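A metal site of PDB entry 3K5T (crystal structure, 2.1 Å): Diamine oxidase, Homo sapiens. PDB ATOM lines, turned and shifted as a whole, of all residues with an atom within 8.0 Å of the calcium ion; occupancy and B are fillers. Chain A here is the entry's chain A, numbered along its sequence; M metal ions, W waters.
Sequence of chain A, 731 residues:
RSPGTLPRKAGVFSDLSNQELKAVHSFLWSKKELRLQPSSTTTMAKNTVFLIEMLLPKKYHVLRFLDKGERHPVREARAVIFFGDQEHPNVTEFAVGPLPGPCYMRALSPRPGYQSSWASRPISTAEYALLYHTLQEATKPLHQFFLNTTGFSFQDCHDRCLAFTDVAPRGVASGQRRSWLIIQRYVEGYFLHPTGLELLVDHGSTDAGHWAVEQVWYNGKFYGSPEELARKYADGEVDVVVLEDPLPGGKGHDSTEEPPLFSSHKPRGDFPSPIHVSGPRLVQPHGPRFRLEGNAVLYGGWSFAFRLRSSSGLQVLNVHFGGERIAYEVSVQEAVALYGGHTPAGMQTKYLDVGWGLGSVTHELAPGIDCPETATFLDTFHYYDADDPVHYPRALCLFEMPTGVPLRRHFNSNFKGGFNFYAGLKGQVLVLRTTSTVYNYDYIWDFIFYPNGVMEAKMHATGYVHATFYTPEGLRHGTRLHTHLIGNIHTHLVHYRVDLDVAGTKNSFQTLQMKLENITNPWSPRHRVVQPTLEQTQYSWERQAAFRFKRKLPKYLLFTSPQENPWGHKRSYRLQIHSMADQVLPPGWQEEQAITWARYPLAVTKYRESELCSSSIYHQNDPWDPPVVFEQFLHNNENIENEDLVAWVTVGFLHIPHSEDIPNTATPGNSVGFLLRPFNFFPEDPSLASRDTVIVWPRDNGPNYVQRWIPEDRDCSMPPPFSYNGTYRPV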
ATOM      1  N   LYS A  59      20.705   8.055  -3.488  1.00  0.00           N
ATOM      2  CA  LYS A  59      19.725   9.095  -3.786  1.00  0.00           C
ATOM      3  C   LYS A  59      18.470   8.509  -4.438  1.00  0.00           C
ATOM      4  O   LYS A  59      17.339   8.945  -4.180  1.00  0.00           O
ATOM      5  CB  LYS A  59      20.351  10.167  -4.681  1.00  0.00           C
ATOM      6  CG  LYS A  59      19.442  11.338  -5.021  1.00  0.00           C
ATOM      7  CD  LYS A  59      20.069  12.225  -6.085  1.00  0.00           C
ATOM      8  CE  LYS A  59      19.366  13.571  -6.144  1.00  0.00           C
ATOM      9  NZ  LYS A  59      19.921  14.501  -7.164  1.00  0.00           N
ATOM     10  N   ARG A 325      10.886  21.005  -4.838  1.00  0.00           N
ATOM     11  CA  ARG A 325      12.296  20.830  -4.501  1.00  0.00           C
ATOM     12  C   ARG A 325      13.154  21.840  -5.248  1.00  0.00           C
ATOM     13  O   ARG A 325      12.815  22.263  -6.357  1.00  0.00           O
ATOM     14  CB  ARG A 325      12.771  19.407  -4.798  1.00  0.00           C
ATOM     15  CG  ARG A 325      14.138  19.104  -4.198  1.00  0.00           C
ATOM     16  CD  ARG A 325      14.466  17.622  -4.355  1.00  0.00           C
ATOM     17  NE  ARG A 325      13.702  16.803  -3.403  1.00  0.00           N
ATOM     18  CZ  ARG A 325      12.928  15.758  -3.692  1.00  0.00           C
ATOM     19  NH1 ARG A 325      12.784  15.305  -4.932  1.00  0.00           N
ATOM     20  NH2 ARG A 325      12.298  15.140  -2.714  1.00  0.00           N
ATOM     21  N   ILE A 326      14.218  22.274  -4.605  1.00  0.00           N
ATOM     22  CA  ILE A 326      15.204  23.116  -5.269  1.00  0.00           C
ATOM     23  C   ILE A 326      16.587  22.503  -5.183  1.00  0.00           C
ATOM     24  O   ILE A 326      17.335  22.540  -6.152  1.00  0.00           O
ATOM     25  CB  ILE A 326      15.191  24.589  -4.771  1.00  0.00           C
ATOM     26  CG1 ILE A 326      16.014  24.762  -3.505  1.00  0.00           C
ATOM     27  CG2 ILE A 326      13.750  25.049  -4.562  1.00  0.00           C
ATOM     28  CD1 ILE A 326      15.942  26.179  -2.894  1.00  0.00           C
ATOM     29  N   ALA A 327      16.907  21.891  -4.038  1.00  0.00           N
ATOM     30  CA  ALA A 327      18.207  21.281  -3.838  1.00  0.00           C
ATOM     31  C   ALA A 327      18.082  19.988  -3.054  1.00  0.00           C
ATOM     32  O   ALA A 327      17.564  19.997  -1.951  1.00  0.00           O
ATOM     33  CB  ALA A 327      19.147  22.272  -3.108  1.00  0.00           C
ATOM     34  N   TYR A 328      18.532  18.878  -3.625  1.00  0.00           N
ATOM     35  CA  TYR A 328      18.648  17.657  -2.848  1.00  0.00           C
ATOM     36  C   TYR A 328      19.688  17.823  -1.716  1.00  0.00           C
ATOM     37  O   TYR A 328      19.472  17.318  -0.613  1.00  0.00           O
ATOM     38  CB  TYR A 328      19.027  16.483  -3.723  1.00  0.00           C
ATOM     39  CG  TYR A 328      19.080  15.182  -2.953  1.00  0.00           C
ATOM     40  CD1 TYR A 328      17.927  14.515  -2.578  1.00  0.00           C
ATOM     41  CD2 TYR A 328      20.291  14.616  -2.589  1.00  0.00           C
ATOM     42  CE1 TYR A 328      17.976  13.315  -1.872  1.00  0.00           C
ATOM     43  CE2 TYR A 328      20.348  13.418  -1.878  1.00  0.00           C
ATOM     44  CZ  TYR A 328      19.195  12.776  -1.530  1.00  0.00           C
ATOM     45  OH  TYR A 328      19.268  11.590  -0.810  1.00  0.00           O
ATOM     46  N   GLU A 329      20.788  18.514  -1.997  1.00  0.00           N
ATOM     47  CA  GLU A 329      21.869  18.688  -1.008  1.00  0.00           C
ATOM     48  C   GLU A 329      22.705  19.936  -1.246  1.00  0.00           C
ATOM     49  O   GLU A 329      23.065  20.225  -2.371  1.00  0.00           O
ATOM     50  CB  GLU A 329      22.810  17.463  -1.024  1.00  0.00           C
ATOM     51  CG  GLU A 329      24.078  17.602  -0.148  1.00  0.00           C
ATOM     52  CD  GLU A 329      25.137  16.549  -0.447  1.00  0.00           C
ATOM     53  OE1 GLU A 329      24.943  15.758  -1.398  1.00  0.00           O
ATOM     54  OE2 GLU A 329      26.197  16.531   0.241  1.00  0.00           O
ATOM     55  N   ARG A 497      29.497  21.435  -2.427  1.00  0.00           N
ATOM     56  CA  ARG A 497      28.766  20.562  -3.337  1.00  0.00           C
ATOM     57  C   ARG A 497      27.322  21.023  -3.335  1.00  0.00           C
ATOM     58  O   ARG A 497      26.667  20.996  -2.305  1.00  0.00           O
ATOM     59  CB  ARG A 497      28.842  19.107  -2.856  1.00  0.00           C
ATOM     60  CG  ARG A 497      27.963  18.143  -3.635  1.00  0.00           C
ATOM     61  CD  ARG A 497      28.087  16.726  -3.032  1.00  0.00           C
ATOM     62  NE  ARG A 497      27.034  15.844  -3.562  1.00  0.00           N
ATOM     63  CZ  ARG A 497      27.114  15.146  -4.695  1.00  0.00           C
ATOM     64  NH1 ARG A 497      28.211  15.177  -5.435  1.00  0.00           N
ATOM     65  NH2 ARG A 497      26.098  14.394  -5.097  1.00  0.00           N
ATOM     66  N   VAL A 498      26.834  21.421  -4.502  1.00  0.00           N
ATOM     67  CA  VAL A 498      25.548  22.094  -4.593  1.00  0.00           C
ATOM     68  C   VAL A 498      24.633  21.312  -5.527  1.00  0.00           C
ATOM     69  O   VAL A 498      24.467  21.648  -6.691  1.00  0.00           O
ATOM     70  CB  VAL A 498      25.739  23.542  -5.076  1.00  0.00           C
ATOM     71  CG1 VAL A 498      24.426  24.315  -5.005  1.00  0.00           C
ATOM     72  CG2 VAL A 498      26.833  24.198  -4.249  1.00  0.00           C
ATOM     73  N   ASP A 499      24.087  20.208  -4.996  1.00  0.00           N
ATOM     74  CA  ASP A 499      23.221  19.319  -5.763  1.00  0.00           C
ATOM     75  C   ASP A 499      21.823  19.937  -5.981  1.00  0.00           C
ATOM     76  O   ASP A 499      20.851  19.490  -5.394  1.00  0.00           O
ATOM     77  CB  ASP A 499      23.134  17.954  -5.053  1.00  0.00           C
ATOM     78  CG  ASP A 499      22.407  16.923  -5.879  1.00  0.00           C
ATOM     79  OD1 ASP A 499      22.039  17.258  -7.008  1.00  0.00           O
ATOM     80  OD2 ASP A 499      22.223  15.766  -5.429  1.00  0.00           O
ATOM     81  N   LEU A 500      21.725  20.965  -6.817  1.00  0.00           N
ATOM     82  CA  LEU A 500      20.443  21.548  -7.169  1.00  0.00           C
ATOM     83  C   LEU A 500      19.580  20.523  -7.953  1.00  0.00           C
ATOM     84  O   LEU A 500      20.065  19.911  -8.879  1.00  0.00           O
ATOM     85  CB  LEU A 500      20.645  22.800  -8.042  1.00  0.00           C
ATOM     86  CG  LEU A 500      21.369  23.996  -7.420  1.00  0.00           C
ATOM     87  CD1 LEU A 500      21.486  25.131  -8.442  1.00  0.00           C
ATOM     88  CD2 LEU A 500      20.635  24.476  -6.207  1.00  0.00           C
ATOM     89  N   ASP A 501      18.342  20.312  -7.500  1.00  0.00           N
ATOM     90  CA  ASP A 501      17.327  19.550  -8.225  1.00  0.00           C
ATOM     91  C   ASP A 501      16.180  20.486  -8.452  1.00  0.00           C
ATOM     92  O   ASP A 501      15.170  20.403  -7.756  1.00  0.00           O
ATOM     93  CB  ASP A 501      16.841  18.352  -7.414  1.00  0.00           C
ATOM     94  CG  ASP A 501      17.803  17.213  -7.416  1.00  0.00           C
ATOM     95  OD1 ASP A 501      18.939  17.397  -7.909  1.00  0.00           O
ATOM     96  OD2 ASP A 501      17.424  16.130  -6.911  1.00  0.00           O
ATOM     97  N   VAL A 502      16.343  21.391  -9.413  1.00  0.00           N
ATOM     98  CA  VAL A 502      15.430  22.522  -9.582  1.00  0.00           C
ATOM     99  C   VAL A 502      14.075  22.043 -10.110  1.00  0.00           C
ATOM    100  O   VAL A 502      13.980  21.493 -11.185  1.00  0.00           O
ATOM    101  CB  VAL A 502      16.006  23.546 -10.552  1.00  0.00           C
ATOM    102  CG1 VAL A 502      15.180  24.824 -10.527  1.00  0.00           C
ATOM    103  CG2 VAL A 502      17.465  23.834 -10.220  1.00  0.00           C
ATOM    104  N   GLY A 504      12.689  19.450  -9.482  1.00  0.00           N
ATOM    105  CA  GLY A 504      12.820  18.012  -9.799  1.00  0.00           C
ATOM    106  C   GLY A 504      14.244  17.567 -10.080  1.00  0.00           C
ATOM    107  O   GLY A 504      15.165  18.374 -10.097  1.00  0.00           O
ATOM    108  N   THR A 505      14.423  16.273 -10.312  1.00  0.00           N
ATOM    109  CA  THR A 505      15.740  15.668 -10.523  1.00  0.00           C
ATOM    110  C   THR A 505      16.439  16.077 -11.826  1.00  0.00           C
ATOM    111  O   THR A 505      17.655  16.290 -11.825  1.00  0.00           O
ATOM    112  CB  THR A 505      15.638  14.144 -10.537  1.00  0.00           C
ATOM    113  OG1 THR A 505      15.062  13.679  -9.314  1.00  0.00           O
ATOM    114  CG2 THR A 505      17.012  13.522 -10.756  1.00  0.00           C
ATOM    115  N   LYS A 506      15.705  16.148 -12.932  1.00  0.00           N
ATOM    116  CA  LYS A 506      16.269  16.440 -14.249  1.00  0.00           C
ATOM    117  C   LYS A 506      16.353  17.939 -14.521  1.00  0.00           C
ATOM    118  O   LYS A 506      15.343  18.636 -14.505  1.00  0.00           O
ATOM    119  CB  LYS A 506      15.416  15.767 -15.337  1.00  0.00           C
ATOM    120  N   ASN A 507      17.557  18.424 -14.803  1.00  0.00           N
ATOM    121  CA  ASN A 507      17.787  19.825 -15.123  1.00  0.00           C
ATOM    122  C   ASN A 507      18.743  19.996 -16.297  1.00  0.00           C
ATOM    123  O   ASN A 507      19.374  19.044 -16.770  1.00  0.00           O
ATOM    124  CB  ASN A 507      18.386  20.568 -13.922  1.00  0.00           C
ATOM    125  CG  ASN A 507      17.433  20.676 -12.732  1.00  0.00           C
ATOM    126  OD1 ASN A 507      17.861  20.588 -11.573  1.00  0.00           O
ATOM    127  ND2 ASN A 507      16.135  20.893 -13.013  1.00  0.00           N
ATOM    128  N   PHE A 559      20.398  27.102 -13.471  1.00  0.00           N
ATOM    129  CA  PHE A 559      20.142  25.666 -13.537  1.00  0.00           C
ATOM    130  C   PHE A 559      18.637  25.554 -13.778  1.00  0.00           C
ATOM    131  O   PHE A 559      17.843  25.952 -12.919  1.00  0.00           O
ATOM    132  CB  PHE A 559      20.584  24.969 -12.253  1.00  0.00           C
ATOM    133  CG  PHE A 559      22.091  24.948 -12.065  1.00  0.00           C
ATOM    134  CD1 PHE A 559      22.791  26.113 -11.756  1.00  0.00           C
ATOM    135  CD2 PHE A 559      22.804  23.763 -12.189  1.00  0.00           C
ATOM    136  CE1 PHE A 559      24.172  26.099 -11.580  1.00  0.00           C
ATOM    137  CE2 PHE A 559      24.194  23.741 -12.006  1.00  0.00           C
ATOM    138  CZ  PHE A 559      24.877  24.903 -11.707  1.00  0.00           C
ATOM    139  N   THR A 605      28.765  18.726 -12.682  1.00  0.00           N
ATOM    140  CA  THR A 605      28.825  17.323 -13.051  1.00  0.00           C
ATOM    141  C   THR A 605      27.451  16.675 -13.112  1.00  0.00           C
ATOM    142  O   THR A 605      26.443  17.200 -12.603  1.00  0.00           O
ATOM    143  CB  THR A 605      29.754  16.495 -12.152  1.00  0.00           C
ATOM    144  OG1 THR A 605      29.223  16.432 -10.831  1.00  0.00           O
ATOM    145  CG2 THR A 605      31.169  17.096 -12.141  1.00  0.00           C
ATOM    146  N   LYS A 606      27.408  15.541 -13.788  1.00  0.00           N
ATOM    147  CA  LYS A 606      26.238  14.702 -13.822  1.00  0.00           C
ATOM    148  C   LYS A 606      26.354  13.836 -12.574  1.00  0.00           C
ATOM    149  O   LYS A 606      27.428  13.319 -12.258  1.00  0.00           O
ATOM    150  CB  LYS A 606      26.257  13.869 -15.098  1.00  0.00           C
ATOM    151  CG  LYS A 606      25.165  12.841 -15.250  1.00  0.00           C
ATOM    152  CD  LYS A 606      24.986  12.504 -16.720  1.00  0.00           C
ATOM    153  CE  LYS A 606      24.665  11.040 -16.958  1.00  0.00           C
ATOM    154  NZ  LYS A 606      25.015  10.692 -18.368  1.00  0.00           N
ATOM    155  N   TYR A 607      25.237  13.718 -11.849  1.00  0.00           N
ATOM    156  CA  TYR A 607      25.208  13.094 -10.546  1.00  0.00           C
ATOM    157  C   TYR A 607      25.665  11.632 -10.610  1.00  0.00           C
ATOM    158  O   TYR A 607      25.335  10.929 -11.566  1.00  0.00           O
ATOM    159  CB  TYR A 607      23.778  13.148  -9.953  1.00  0.00           C
ATOM    160  CG  TYR A 607      23.686  12.429  -8.632  1.00  0.00           C
ATOM    161  CD1 TYR A 607      23.499  11.034  -8.574  1.00  0.00           C
ATOM    162  CD2 TYR A 607      23.849  13.119  -7.447  1.00  0.00           C
ATOM    163  CE1 TYR A 607      23.452  10.370  -7.363  1.00  0.00           C
ATOM    164  CE2 TYR A 607      23.796  12.467  -6.229  1.00  0.00           C
ATOM    165  CZ  TYR A 607      23.611  11.109  -6.186  1.00  0.00           C
ATOM    166  OH  TYR A 607      23.586  10.512  -4.957  1.00  0.00           O
ATOM    167  N   GLU A 643      19.636  16.203 -17.168  1.00  0.00           N
ATOM    168  CA  GLU A 643      20.126  15.133 -16.310  1.00  0.00           C
ATOM    169  C   GLU A 643      20.182  15.626 -14.868  1.00  0.00           C
ATOM    170  O   GLU A 643      20.052  16.835 -14.629  1.00  0.00           O
ATOM    171  CB  GLU A 643      21.518  14.683 -16.768  1.00  0.00           C
ATOM    172  CG  GLU A 643      21.590  14.048 -18.155  1.00  0.00           C
ATOM    173  CD  GLU A 643      21.058  12.617 -18.223  1.00  0.00           C
ATOM    174  OE1 GLU A 643      21.048  11.903 -17.186  1.00  0.00           O
ATOM    175  OE2 GLU A 643      20.640  12.196 -19.323  1.00  0.00           O
ATOM    176  N   ASP A 644      20.353  14.705 -13.937  1.00  0.00           N
ATOM    177  CA  ASP A 644      20.620  15.038 -12.529  1.00  0.00           C
ATOM    178  C   ASP A 644      21.996  15.724 -12.483  1.00  0.00           C
ATOM    179  O   ASP A 644      23.047  15.072 -12.599  1.00  0.00           O
ATOM    180  CB  ASP A 644      20.582  13.762 -11.641  1.00  0.00           C
ATOM    181  CG  ASP A 644      20.443  14.060 -10.111  1.00  0.00           C
ATOM    182  OD1 ASP A 644      20.591  15.230  -9.671  1.00  0.00           O
ATOM    183  OD2 ASP A 644      20.219  13.093  -9.337  1.00  0.00           O
ATOM    184  N   LEU A 645      21.967  17.048 -12.385  1.00  0.00           N
ATOM    185  CA  LEU A 645      23.173  17.864 -12.324  1.00  0.00           C
ATOM    186  C   LEU A 645      23.582  18.136 -10.874  1.00  0.00           C
ATOM    187  O   LEU A 645      22.740  18.241  -9.973  1.00  0.00           O
ATOM    188  CB  LEU A 645      22.966  19.225 -13.022  1.00  0.00           C
ATOM    189  CG  LEU A 645      22.578  19.277 -14.500  1.00  0.00           C
ATOM    190  CD1 LEU A 645      22.692  20.729 -15.035  1.00  0.00           C
ATOM    191  CD2 LEU A 645      23.433  18.346 -15.298  1.00  0.00           C
ATOM    192  N   VAL A 646      24.890  18.290 -10.696  1.00  0.00           N
ATOM    193  CA  VAL A 646      25.499  18.687  -9.432  1.00  0.00           C
ATOM    194  C   VAL A 646      26.425  19.876  -9.699  1.00  0.00           C
ATOM    195  O   VAL A 646      27.318  19.789 -10.534  1.00  0.00           O
ATOM    196  CB  VAL A 646      26.299  17.526  -8.827  1.00  0.00           C
ATOM    197  CG1 VAL A 646      27.050  17.972  -7.596  1.00  0.00           C
ATOM    198  CG2 VAL A 646      25.377  16.337  -8.509  1.00  0.00           C
ATOM    199  N   ALA A 647      26.203  20.987  -9.014  1.00  0.00           N
ATOM    200  CA  ALA A 647      27.110  22.123  -9.119  1.00  0.00           C
ATOM    201  C   ALA A 647      28.191  21.967  -8.039  1.00  0.00           C
ATOM    202  O   ALA A 647      27.940  21.400  -6.974  1.00  0.00           O
ATOM    203  CB  ALA A 647      26.356  23.412  -8.964  1.00  0.00           C
HETATM  204 CA    CA M   1      20.738  17.608  -9.004  1.00  0.00          CA
HETATM  205  O   HOH W   1      19.477  18.331 -11.589  1.00  0.00           O
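The backbone NH (N) of Asp 501 is in hydrogen-bond range of the backbone carbonyl oxygen (O) of Ile 326. O of Asp 644 is in hydrogen-bond range of N of Tyr 607 (2.7 Å). The backbone NH (N) of Tyr 328 sits at hydrogen-bond distance from the backbone carbonyl oxygen (O) of Asp 499 (3.0 Å). The backbone carbonyl oxygen of Glu 329 lies within hydrogen-bond range of the backbone NH of Asp 499 (2.8 Å). The side-chain carboxylate (OD2) of Asp 499 is in salt-bridge range of the side-chain amino group (NZ) of Lys 59 (3.1 Å). NZ of Lys 59 is in salt-bridge range of OD2 of Asp 501, at 3.0 Å. OD2 of Asp 644 lies within salt-bridge range of NZ of Lys 59, 2.6 Å away.
The calcium ion is bound by OD1 of Asp 501 (2.1 Å), O of Leu 645 (2.3 Å), O of Leu 500 (2.4 Å), OD1 of Asp 499 (2.4 Å) and OD1 of Asp 644 (2.5 Å). Slightly farther from the calcium ion lies water W1 (3.0 Å).
Residues that only touch the calcium ion: Lys 59 (3.7 Å). Of the 25 residues printed, 6 come within 4 Å of the calcium ion.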
